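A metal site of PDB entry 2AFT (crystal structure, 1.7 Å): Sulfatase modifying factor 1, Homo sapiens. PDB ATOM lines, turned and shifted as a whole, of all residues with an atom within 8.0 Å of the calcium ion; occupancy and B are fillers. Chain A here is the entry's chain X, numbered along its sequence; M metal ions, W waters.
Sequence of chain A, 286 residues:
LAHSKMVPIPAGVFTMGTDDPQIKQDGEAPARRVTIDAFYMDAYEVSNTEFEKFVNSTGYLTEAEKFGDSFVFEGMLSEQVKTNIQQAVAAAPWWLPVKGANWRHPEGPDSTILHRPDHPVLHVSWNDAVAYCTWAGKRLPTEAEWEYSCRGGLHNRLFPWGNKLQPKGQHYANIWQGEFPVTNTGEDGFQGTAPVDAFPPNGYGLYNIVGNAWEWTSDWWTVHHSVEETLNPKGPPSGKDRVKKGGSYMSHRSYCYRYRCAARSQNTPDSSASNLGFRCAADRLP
Ile 209 touches the calcium ion.
Within 4 Å of the calcium ion: Glu 45, Asn 208, Ile 209, Gly 211, Ala 213 and Glu 215.
The nearest printed residue that does not touch the calcium ion is Asn 212 (4.4 Å).
The indole nitrogen (NE1) of Trp 146 sits at hydrogen-bond distance from the side-chain carboxylate (OE1) of Glu 215.
The backbone carbonyl oxygen of Gly 246 sits at hydrogen-bond distance from the backbone NH of Gly 211 (2.8 Å).
The guanidinium group of Arg 279 lies within salt-bridge range of the side-chain carboxylate of Glu 215, at 2.8 Å.
The side-chain amide nitrogen (ND2) of Asn 212 lies within hydrogen-bond range of the side-chain carboxylate (OE1) of Glu 45, 2.8 Å away.
NH2 of Arg 279 sits close to O of Asn 208.
The backbone NH (N) of Lys 245 is in hydrogen-bond range of the backbone carbonyl oxygen (O) of Glu 215.
The calcium ion is bound by water W1 (2.3 Å), OE2 of Glu 215 (2.4 Å), O of Ala 213 (2.4 Å), OE2 of Glu 45 (2.4 Å), O of Asn 208 (2.4 Å) and O of Gly 211 (2.4 Å).
The calcium ion has six donor atoms within binding distance.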
ATOM      1  N   TYR A  44     -23.135 -25.798 -16.101  1.00  0.00           N
ATOM      2  CA  TYR A  44     -21.743 -25.650 -15.662  1.00  0.00           C
ATOM      3  C   TYR A  44     -21.668 -25.121 -14.234  1.00  0.00           C
ATOM      4  O   TYR A  44     -22.529 -24.376 -13.800  1.00  0.00           O
ATOM      5  CB  TYR A  44     -21.050 -24.591 -16.539  1.00  0.00           C
ATOM      6  CG  TYR A  44     -21.167 -24.826 -18.018  1.00  0.00           C
ATOM      7  CD1 TYR A  44     -20.518 -25.896 -18.613  1.00  0.00           C
ATOM      8  CD2 TYR A  44     -21.947 -23.976 -18.825  1.00  0.00           C
ATOM      9  CE1 TYR A  44     -20.610 -26.114 -19.965  1.00  0.00           C
ATOM     10  CE2 TYR A  44     -22.043 -24.186 -20.172  1.00  0.00           C
ATOM     11  CZ  TYR A  44     -21.368 -25.257 -20.743  1.00  0.00           C
ATOM     12  OH  TYR A  44     -21.451 -25.501 -22.107  1.00  0.00           O
ATOM     13  N   GLU A  45     -20.629 -25.503 -13.490  1.00  0.00           N
ATOM     14  CA  GLU A  45     -20.268 -24.811 -12.279  1.00  0.00           C
ATOM     15  C   GLU A  45     -20.120 -23.332 -12.628  1.00  0.00           C
ATOM     16  O   GLU A  45     -19.737 -23.004 -13.741  1.00  0.00           O
ATOM     17  CB  GLU A  45     -18.931 -25.318 -11.760  1.00  0.00           C
ATOM     18  CG  GLU A  45     -18.935 -26.792 -11.355  1.00  0.00           C
ATOM     19  CD  GLU A  45     -17.556 -27.476 -11.400  1.00  0.00           C
ATOM     20  OE1 GLU A  45     -16.773 -27.213 -12.346  1.00  0.00           O
ATOM     21  OE2 GLU A  45     -17.287 -28.327 -10.523  1.00  0.00           O
ATOM     22  N   PRO A 120     -14.009 -23.059 -12.459  1.00  0.00           N
ATOM     23  CA  PRO A 120     -15.010 -22.801 -11.449  1.00  0.00           C
ATOM     24  C   PRO A 120     -14.515 -21.827 -10.409  1.00  0.00           C
ATOM     25  O   PRO A 120     -13.357 -21.869  -9.991  1.00  0.00           O
ATOM     26  CB  PRO A 120     -15.252 -24.189 -10.810  1.00  0.00           C
ATOM     27  CG  PRO A 120     -13.990 -24.924 -11.036  1.00  0.00           C
ATOM     28  CD  PRO A 120     -13.566 -24.469 -12.419  1.00  0.00           C
ATOM     29  N   TRP A 146     -30.163 -31.753  -6.822  1.00  0.00           N
ATOM     30  CA  TRP A 146     -28.768 -31.902  -7.236  1.00  0.00           C
ATOM     31  C   TRP A 146     -28.454 -33.373  -7.558  1.00  0.00           C
ATOM     32  O   TRP A 146     -27.859 -33.714  -8.610  1.00  0.00           O
ATOM     33  CB  TRP A 146     -27.812 -31.349  -6.149  1.00  0.00           C
ATOM     34  CG  TRP A 146     -26.376 -31.295  -6.630  1.00  0.00           C
ATOM     35  CD1 TRP A 146     -25.688 -30.199  -7.061  1.00  0.00           C
ATOM     36  CD2 TRP A 146     -25.466 -32.405  -6.742  1.00  0.00           C
ATOM     37  NE1 TRP A 146     -24.413 -30.549  -7.429  1.00  0.00           N
ATOM     38  CE2 TRP A 146     -24.259 -31.893  -7.254  1.00  0.00           C
ATOM     39  CE3 TRP A 146     -25.555 -33.769  -6.483  1.00  0.00           C
ATOM     40  CZ2 TRP A 146     -23.163 -32.704  -7.509  1.00  0.00           C
ATOM     41  CZ3 TRP A 146     -24.470 -34.569  -6.746  1.00  0.00           C
ATOM     42  CH2 TRP A 146     -23.288 -34.040  -7.262  1.00  0.00           C
ATOM     43  N   ASN A 174     -12.802 -34.780 -13.384  1.00  0.00           N
ATOM     44  CA  ASN A 174     -11.540 -34.313 -12.855  1.00  0.00           C
ATOM     45  C   ASN A 174     -11.448 -34.619 -11.356  1.00  0.00           C
ATOM     46  O   ASN A 174     -11.987 -33.911 -10.543  1.00  0.00           O
ATOM     47  CB  ASN A 174     -11.389 -32.818 -13.114  1.00  0.00           C
ATOM     48  CG  ASN A 174     -10.109 -32.253 -12.552  1.00  0.00           C
ATOM     49  OD1 ASN A 174      -9.150 -33.028 -12.346  1.00  0.00           O
ATOM     50  ND2 ASN A 174     -10.068 -30.932 -12.289  1.00  0.00           N
ATOM     51  N   TYR A 207     -22.076 -30.663 -16.943  1.00  0.00           N
ATOM     52  CA  TYR A 207     -20.633 -30.854 -16.949  1.00  0.00           C
ATOM     53  C   TYR A 207     -20.091 -30.805 -15.517  1.00  0.00           C
ATOM     54  O   TYR A 207     -20.504 -29.941 -14.726  1.00  0.00           O
ATOM     55  CB  TYR A 207     -19.949 -29.761 -17.784  1.00  0.00           C
ATOM     56  CG  TYR A 207     -20.292 -29.846 -19.245  1.00  0.00           C
ATOM     57  CD1 TYR A 207     -21.534 -29.434 -19.712  1.00  0.00           C
ATOM     58  CD2 TYR A 207     -19.406 -30.447 -20.138  1.00  0.00           C
ATOM     59  CE1 TYR A 207     -21.886 -29.561 -21.024  1.00  0.00           C
ATOM     60  CE2 TYR A 207     -19.733 -30.573 -21.504  1.00  0.00           C
ATOM     61  CZ  TYR A 207     -20.970 -30.127 -21.939  1.00  0.00           C
ATOM     62  OH  TYR A 207     -21.303 -30.259 -23.275  1.00  0.00           O
ATOM     63  N   ASN A 208     -19.158 -31.715 -15.205  1.00  0.00           N
ATOM     64  CA  ASN A 208     -18.377 -31.644 -13.958  1.00  0.00           C
ATOM     65  C   ASN A 208     -19.267 -31.682 -12.717  1.00  0.00           C
ATOM     66  O   ASN A 208     -18.927 -31.113 -11.703  1.00  0.00           O
ATOM     67  CB  ASN A 208     -17.451 -30.426 -13.968  1.00  0.00           C
ATOM     68  CG  ASN A 208     -16.459 -30.541 -15.084  1.00  0.00           C
ATOM     69  OD1 ASN A 208     -15.682 -31.505 -15.121  1.00  0.00           O
ATOM     70  ND2 ASN A 208     -16.560 -29.657 -16.058  1.00  0.00           N
ATOM     71  N   ILE A 209     -20.376 -32.403 -12.826  1.00  0.00           N
ATOM     72  CA  ILE A 209     -21.299 -32.534 -11.687  1.00  0.00           C
ATOM     73  C   ILE A 209     -20.665 -33.422 -10.586  1.00  0.00           C
ATOM     74  O   ILE A 209     -20.842 -33.156  -9.428  1.00  0.00           O
ATOM     75  CB  ILE A 209     -22.711 -32.978 -12.119  1.00  0.00           C
ATOM     76  CG1 ILE A 209     -23.688 -32.886 -10.922  1.00  0.00           C
ATOM     77  CG2 ILE A 209     -22.683 -34.351 -12.700  1.00  0.00           C
ATOM     78  CD1 ILE A 209     -24.383 -31.669 -10.802  1.00  0.00           C
ATOM     79  N   VAL A 210     -19.872 -34.428 -10.955  1.00  0.00           N
ATOM     80  CA  VAL A 210     -18.907 -35.021 -10.016  1.00  0.00           C
ATOM     81  C   VAL A 210     -17.497 -34.532 -10.387  1.00  0.00           C
ATOM     82  O   VAL A 210     -17.182 -34.278 -11.573  1.00  0.00           O
ATOM     83  CB  VAL A 210     -18.946 -36.563  -9.883  1.00  0.00           C
ATOM     84  CG1 VAL A 210     -20.311 -37.006  -9.446  1.00  0.00           C
ATOM     85  CG2 VAL A 210     -18.565 -37.253 -11.144  1.00  0.00           C
ATOM     86  N   GLY A 211     -16.684 -34.350  -9.362  1.00  0.00           N
ATOM     87  CA  GLY A 211     -15.322 -33.848  -9.537  1.00  0.00           C
ATOM     88  C   GLY A 211     -15.228 -32.350  -9.824  1.00  0.00           C
ATOM     89  O   GLY A 211     -16.239 -31.608  -9.814  1.00  0.00           O
ATOM     90  N   ASN A 212     -13.991 -31.904 -10.035  1.00  0.00           N
ATOM     91  CA  ASN A 212     -13.660 -30.496 -10.284  1.00  0.00           C
ATOM     92  C   ASN A 212     -13.835 -29.674  -9.002  1.00  0.00           C
ATOM     93  O   ASN A 212     -12.953 -29.768  -8.155  1.00  0.00           O
ATOM     94  CB  ASN A 212     -14.386 -29.916 -11.532  1.00  0.00           C
ATOM     95  CG  ASN A 212     -13.501 -28.908 -12.318  1.00  0.00           C
ATOM     96  OD1 ASN A 212     -12.288 -29.076 -12.365  1.00  0.00           O
ATOM     97  ND2 ASN A 212     -14.121 -27.885 -12.940  1.00  0.00           N
ATOM     98  N   ALA A 213     -14.936 -28.940  -8.812  1.00  0.00           N
ATOM     99  CA  ALA A 213     -15.226 -28.267  -7.514  1.00  0.00           C
ATOM    100  C   ALA A 213     -16.388 -29.024  -6.856  1.00  0.00           C
ATOM    101  O   ALA A 213     -17.297 -29.518  -7.548  1.00  0.00           O
ATOM    102  CB  ALA A 213     -15.619 -26.847  -7.749  1.00  0.00           C
ATOM    103  N   TRP A 214     -16.309 -29.162  -5.541  1.00  0.00           N
ATOM    104  CA  TRP A 214     -17.478 -29.494  -4.719  1.00  0.00           C
ATOM    105  C   TRP A 214     -18.584 -28.471  -5.014  1.00  0.00           C
ATOM    106  O   TRP A 214     -18.301 -27.323  -5.424  1.00  0.00           O
ATOM    107  CB  TRP A 214     -17.140 -29.377  -3.229  1.00  0.00           C
ATOM    108  CG  TRP A 214     -16.538 -30.571  -2.613  1.00  0.00           C
ATOM    109  CD1 TRP A 214     -15.208 -30.769  -2.361  1.00  0.00           C
ATOM    110  CD2 TRP A 214     -17.227 -31.725  -2.088  1.00  0.00           C
ATOM    111  NE1 TRP A 214     -15.019 -31.991  -1.734  1.00  0.00           N
ATOM    112  CE2 TRP A 214     -16.236 -32.613  -1.583  1.00  0.00           C
ATOM    113  CE3 TRP A 214     -18.561 -32.115  -2.043  1.00  0.00           C
ATOM    114  CZ2 TRP A 214     -16.568 -33.855  -1.025  1.00  0.00           C
ATOM    115  CZ3 TRP A 214     -18.887 -33.374  -1.493  1.00  0.00           C
ATOM    116  CH2 TRP A 214     -17.888 -34.213  -0.984  1.00  0.00           C
ATOM    117  N   GLU A 215     -19.830 -28.840  -4.728  1.00  0.00           N
ATOM    118  CA  GLU A 215     -20.943 -27.967  -5.015  1.00  0.00           C
ATOM    119  C   GLU A 215     -21.913 -27.818  -3.854  1.00  0.00           C
ATOM    120  O   GLU A 215     -22.443 -28.802  -3.330  1.00  0.00           O
ATOM    121  CB  GLU A 215     -21.649 -28.490  -6.294  1.00  0.00           C
ATOM    122  CG  GLU A 215     -20.692 -28.467  -7.453  1.00  0.00           C
ATOM    123  CD  GLU A 215     -21.241 -28.978  -8.774  1.00  0.00           C
ATOM    124  OE1 GLU A 215     -22.469 -29.075  -8.922  1.00  0.00           O
ATOM    125  OE2 GLU A 215     -20.400 -29.295  -9.653  1.00  0.00           O
ATOM    126  N   LYS A 245     -22.032 -31.464  -2.375  1.00  0.00           N
ATOM    127  CA  LYS A 245     -22.098 -32.683  -3.148  1.00  0.00           C
ATOM    128  C   LYS A 245     -21.033 -32.733  -4.241  1.00  0.00           C
ATOM    129  O   LYS A 245     -20.563 -31.690  -4.719  1.00  0.00           O
ATOM    130  CB  LYS A 245     -23.467 -32.820  -3.831  1.00  0.00           C
ATOM    131  CG  LYS A 245     -24.683 -32.899  -2.886  1.00  0.00           C
ATOM    132  CD  LYS A 245     -24.840 -34.243  -2.245  1.00  0.00           C
ATOM    133  CE  LYS A 245     -25.639 -35.223  -3.111  1.00  0.00           C
ATOM    134  NZ  LYS A 245     -25.992 -36.528  -2.418  1.00  0.00           N
ATOM    135  N   GLY A 246     -20.694 -33.953  -4.617  1.00  0.00           N
ATOM    136  CA  GLY A 246     -20.088 -34.257  -5.900  1.00  0.00           C
ATOM    137  C   GLY A 246     -18.582 -34.493  -5.933  1.00  0.00           C
ATOM    138  O   GLY A 246     -18.059 -34.940  -6.973  1.00  0.00           O
ATOM    139  N   GLY A 247     -17.874 -34.184  -4.841  1.00  0.00           N
ATOM    140  CA  GLY A 247     -16.425 -34.365  -4.840  1.00  0.00           C
ATOM    141  C   GLY A 247     -15.741 -33.289  -5.662  1.00  0.00           C
ATOM    142  O   GLY A 247     -16.388 -32.383  -6.191  1.00  0.00           O
ATOM    143  N   SER A 248     -14.409 -33.409  -5.758  1.00  0.00           N
ATOM    144  CA  SER A 248     -13.583 -32.409  -6.362  1.00  0.00           C
ATOM    145  C   SER A 248     -12.355 -33.025  -7.044  1.00  0.00           C
ATOM    146  O   SER A 248     -12.151 -34.228  -6.991  1.00  0.00           O
ATOM    147  CB  SER A 248     -13.107 -31.431  -5.299  1.00  0.00           C
ATOM    148  OG  SER A 248     -12.070 -32.016  -4.507  1.00  0.00           O
ATOM    149  N   TYR A 249     -11.528 -32.154  -7.604  1.00  0.00           N
ATOM    150  CA  TYR A 249     -10.228 -32.547  -8.177  1.00  0.00           C
ATOM    151  C   TYR A 249      -9.264 -33.218  -7.200  1.00  0.00           C
ATOM    152  O   TYR A 249      -8.279 -33.838  -7.618  1.00  0.00           O
ATOM    153  CB  TYR A 249      -9.553 -31.338  -8.823  1.00  0.00           C
ATOM    154  CG  TYR A 249      -9.067 -30.243  -7.867  1.00  0.00           C
ATOM    155  CD1 TYR A 249      -9.796 -29.052  -7.674  1.00  0.00           C
ATOM    156  CD2 TYR A 249      -7.860 -30.376  -7.228  1.00  0.00           C
ATOM    157  CE1 TYR A 249      -9.304 -28.036  -6.818  1.00  0.00           C
ATOM    158  CE2 TYR A 249      -7.351 -29.369  -6.386  1.00  0.00           C
ATOM    159  CZ  TYR A 249      -8.077 -28.209  -6.176  1.00  0.00           C
ATOM    160  OH  TYR A 249      -7.523 -27.237  -5.348  1.00  0.00           O
ATOM    161  N   ASN A 275     -11.373 -25.978  -3.037  1.00  0.00           N
ATOM    162  CA  ASN A 275     -11.958 -27.054  -3.847  1.00  0.00           C
ATOM    163  C   ASN A 275     -13.485 -27.042  -3.836  1.00  0.00           C
ATOM    164  O   ASN A 275     -14.122 -28.056  -4.170  1.00  0.00           O
ATOM    165  CB  ASN A 275     -11.477 -28.415  -3.373  1.00  0.00           C
ATOM    166  CG  ASN A 275     -12.038 -28.801  -2.027  1.00  0.00           C
ATOM    167  OD1 ASN A 275     -12.570 -27.963  -1.325  1.00  0.00           O
ATOM    168  ND2 ASN A 275     -11.864 -30.104  -1.654  1.00  0.00           N
ATOM    169  N   GLY A 277     -17.061 -24.934  -4.815  1.00  0.00           N
ATOM    170  CA  GLY A 277     -17.789 -23.955  -5.625  1.00  0.00           C
ATOM    171  C   GLY A 277     -19.268 -24.295  -5.607  1.00  0.00           C
ATOM    172  O   GLY A 277     -19.816 -24.769  -4.573  1.00  0.00           O
ATOM    173  N   PHE A 278     -19.916 -24.016  -6.735  1.00  0.00           N
ATOM    174  CA  PHE A 278     -21.361 -24.234  -6.840  1.00  0.00           C
ATOM    175  C   PHE A 278     -21.876 -24.049  -8.243  1.00  0.00           C
ATOM    176  O   PHE A 278     -21.187 -23.490  -9.097  1.00  0.00           O
ATOM    177  CB  PHE A 278     -22.135 -23.266  -5.926  1.00  0.00           C
ATOM    178  CG  PHE A 278     -22.048 -21.817  -6.334  1.00  0.00           C
ATOM    179  CD1 PHE A 278     -23.135 -21.178  -6.918  1.00  0.00           C
ATOM    180  CD2 PHE A 278     -20.939 -21.060  -6.033  1.00  0.00           C
ATOM    181  CE1 PHE A 278     -23.083 -19.811  -7.238  1.00  0.00           C
ATOM    182  CE2 PHE A 278     -20.860 -19.705  -6.402  1.00  0.00           C
ATOM    183  CZ  PHE A 278     -21.941 -19.087  -6.986  1.00  0.00           C
ATOM    184  N   ARG A 279     -23.121 -24.488  -8.433  1.00  0.00           N
ATOM    185  CA  ARG A 279     -23.921 -24.138  -9.587  1.00  0.00           C
ATOM    186  C   ARG A 279     -25.331 -23.784  -9.119  1.00  0.00           C
ATOM    187  O   ARG A 279     -25.737 -24.141  -8.014  1.00  0.00           O
ATOM    188  CB  ARG A 279     -23.978 -25.261 -10.594  1.00  0.00           C
ATOM    189  CG  ARG A 279     -24.890 -26.411 -10.234  1.00  0.00           C
ATOM    190  CD  ARG A 279     -24.839 -27.498 -11.321  1.00  0.00           C
ATOM    191  NE  ARG A 279     -23.549 -28.195 -11.339  1.00  0.00           N
ATOM    192  CZ  ARG A 279     -22.865 -28.555 -12.424  1.00  0.00           C
ATOM    193  NH1 ARG A 279     -23.304 -28.293 -13.637  1.00  0.00           N
ATOM    194  NH2 ARG A 279     -21.717 -29.195 -12.292  1.00  0.00           N
HETATM  195 CA    CA M   1     -18.255 -30.259  -9.567  1.00  0.00          CA
HETATM  196  O   HOH W   1     -18.851 -31.837  -7.976  1.00  0.00           O
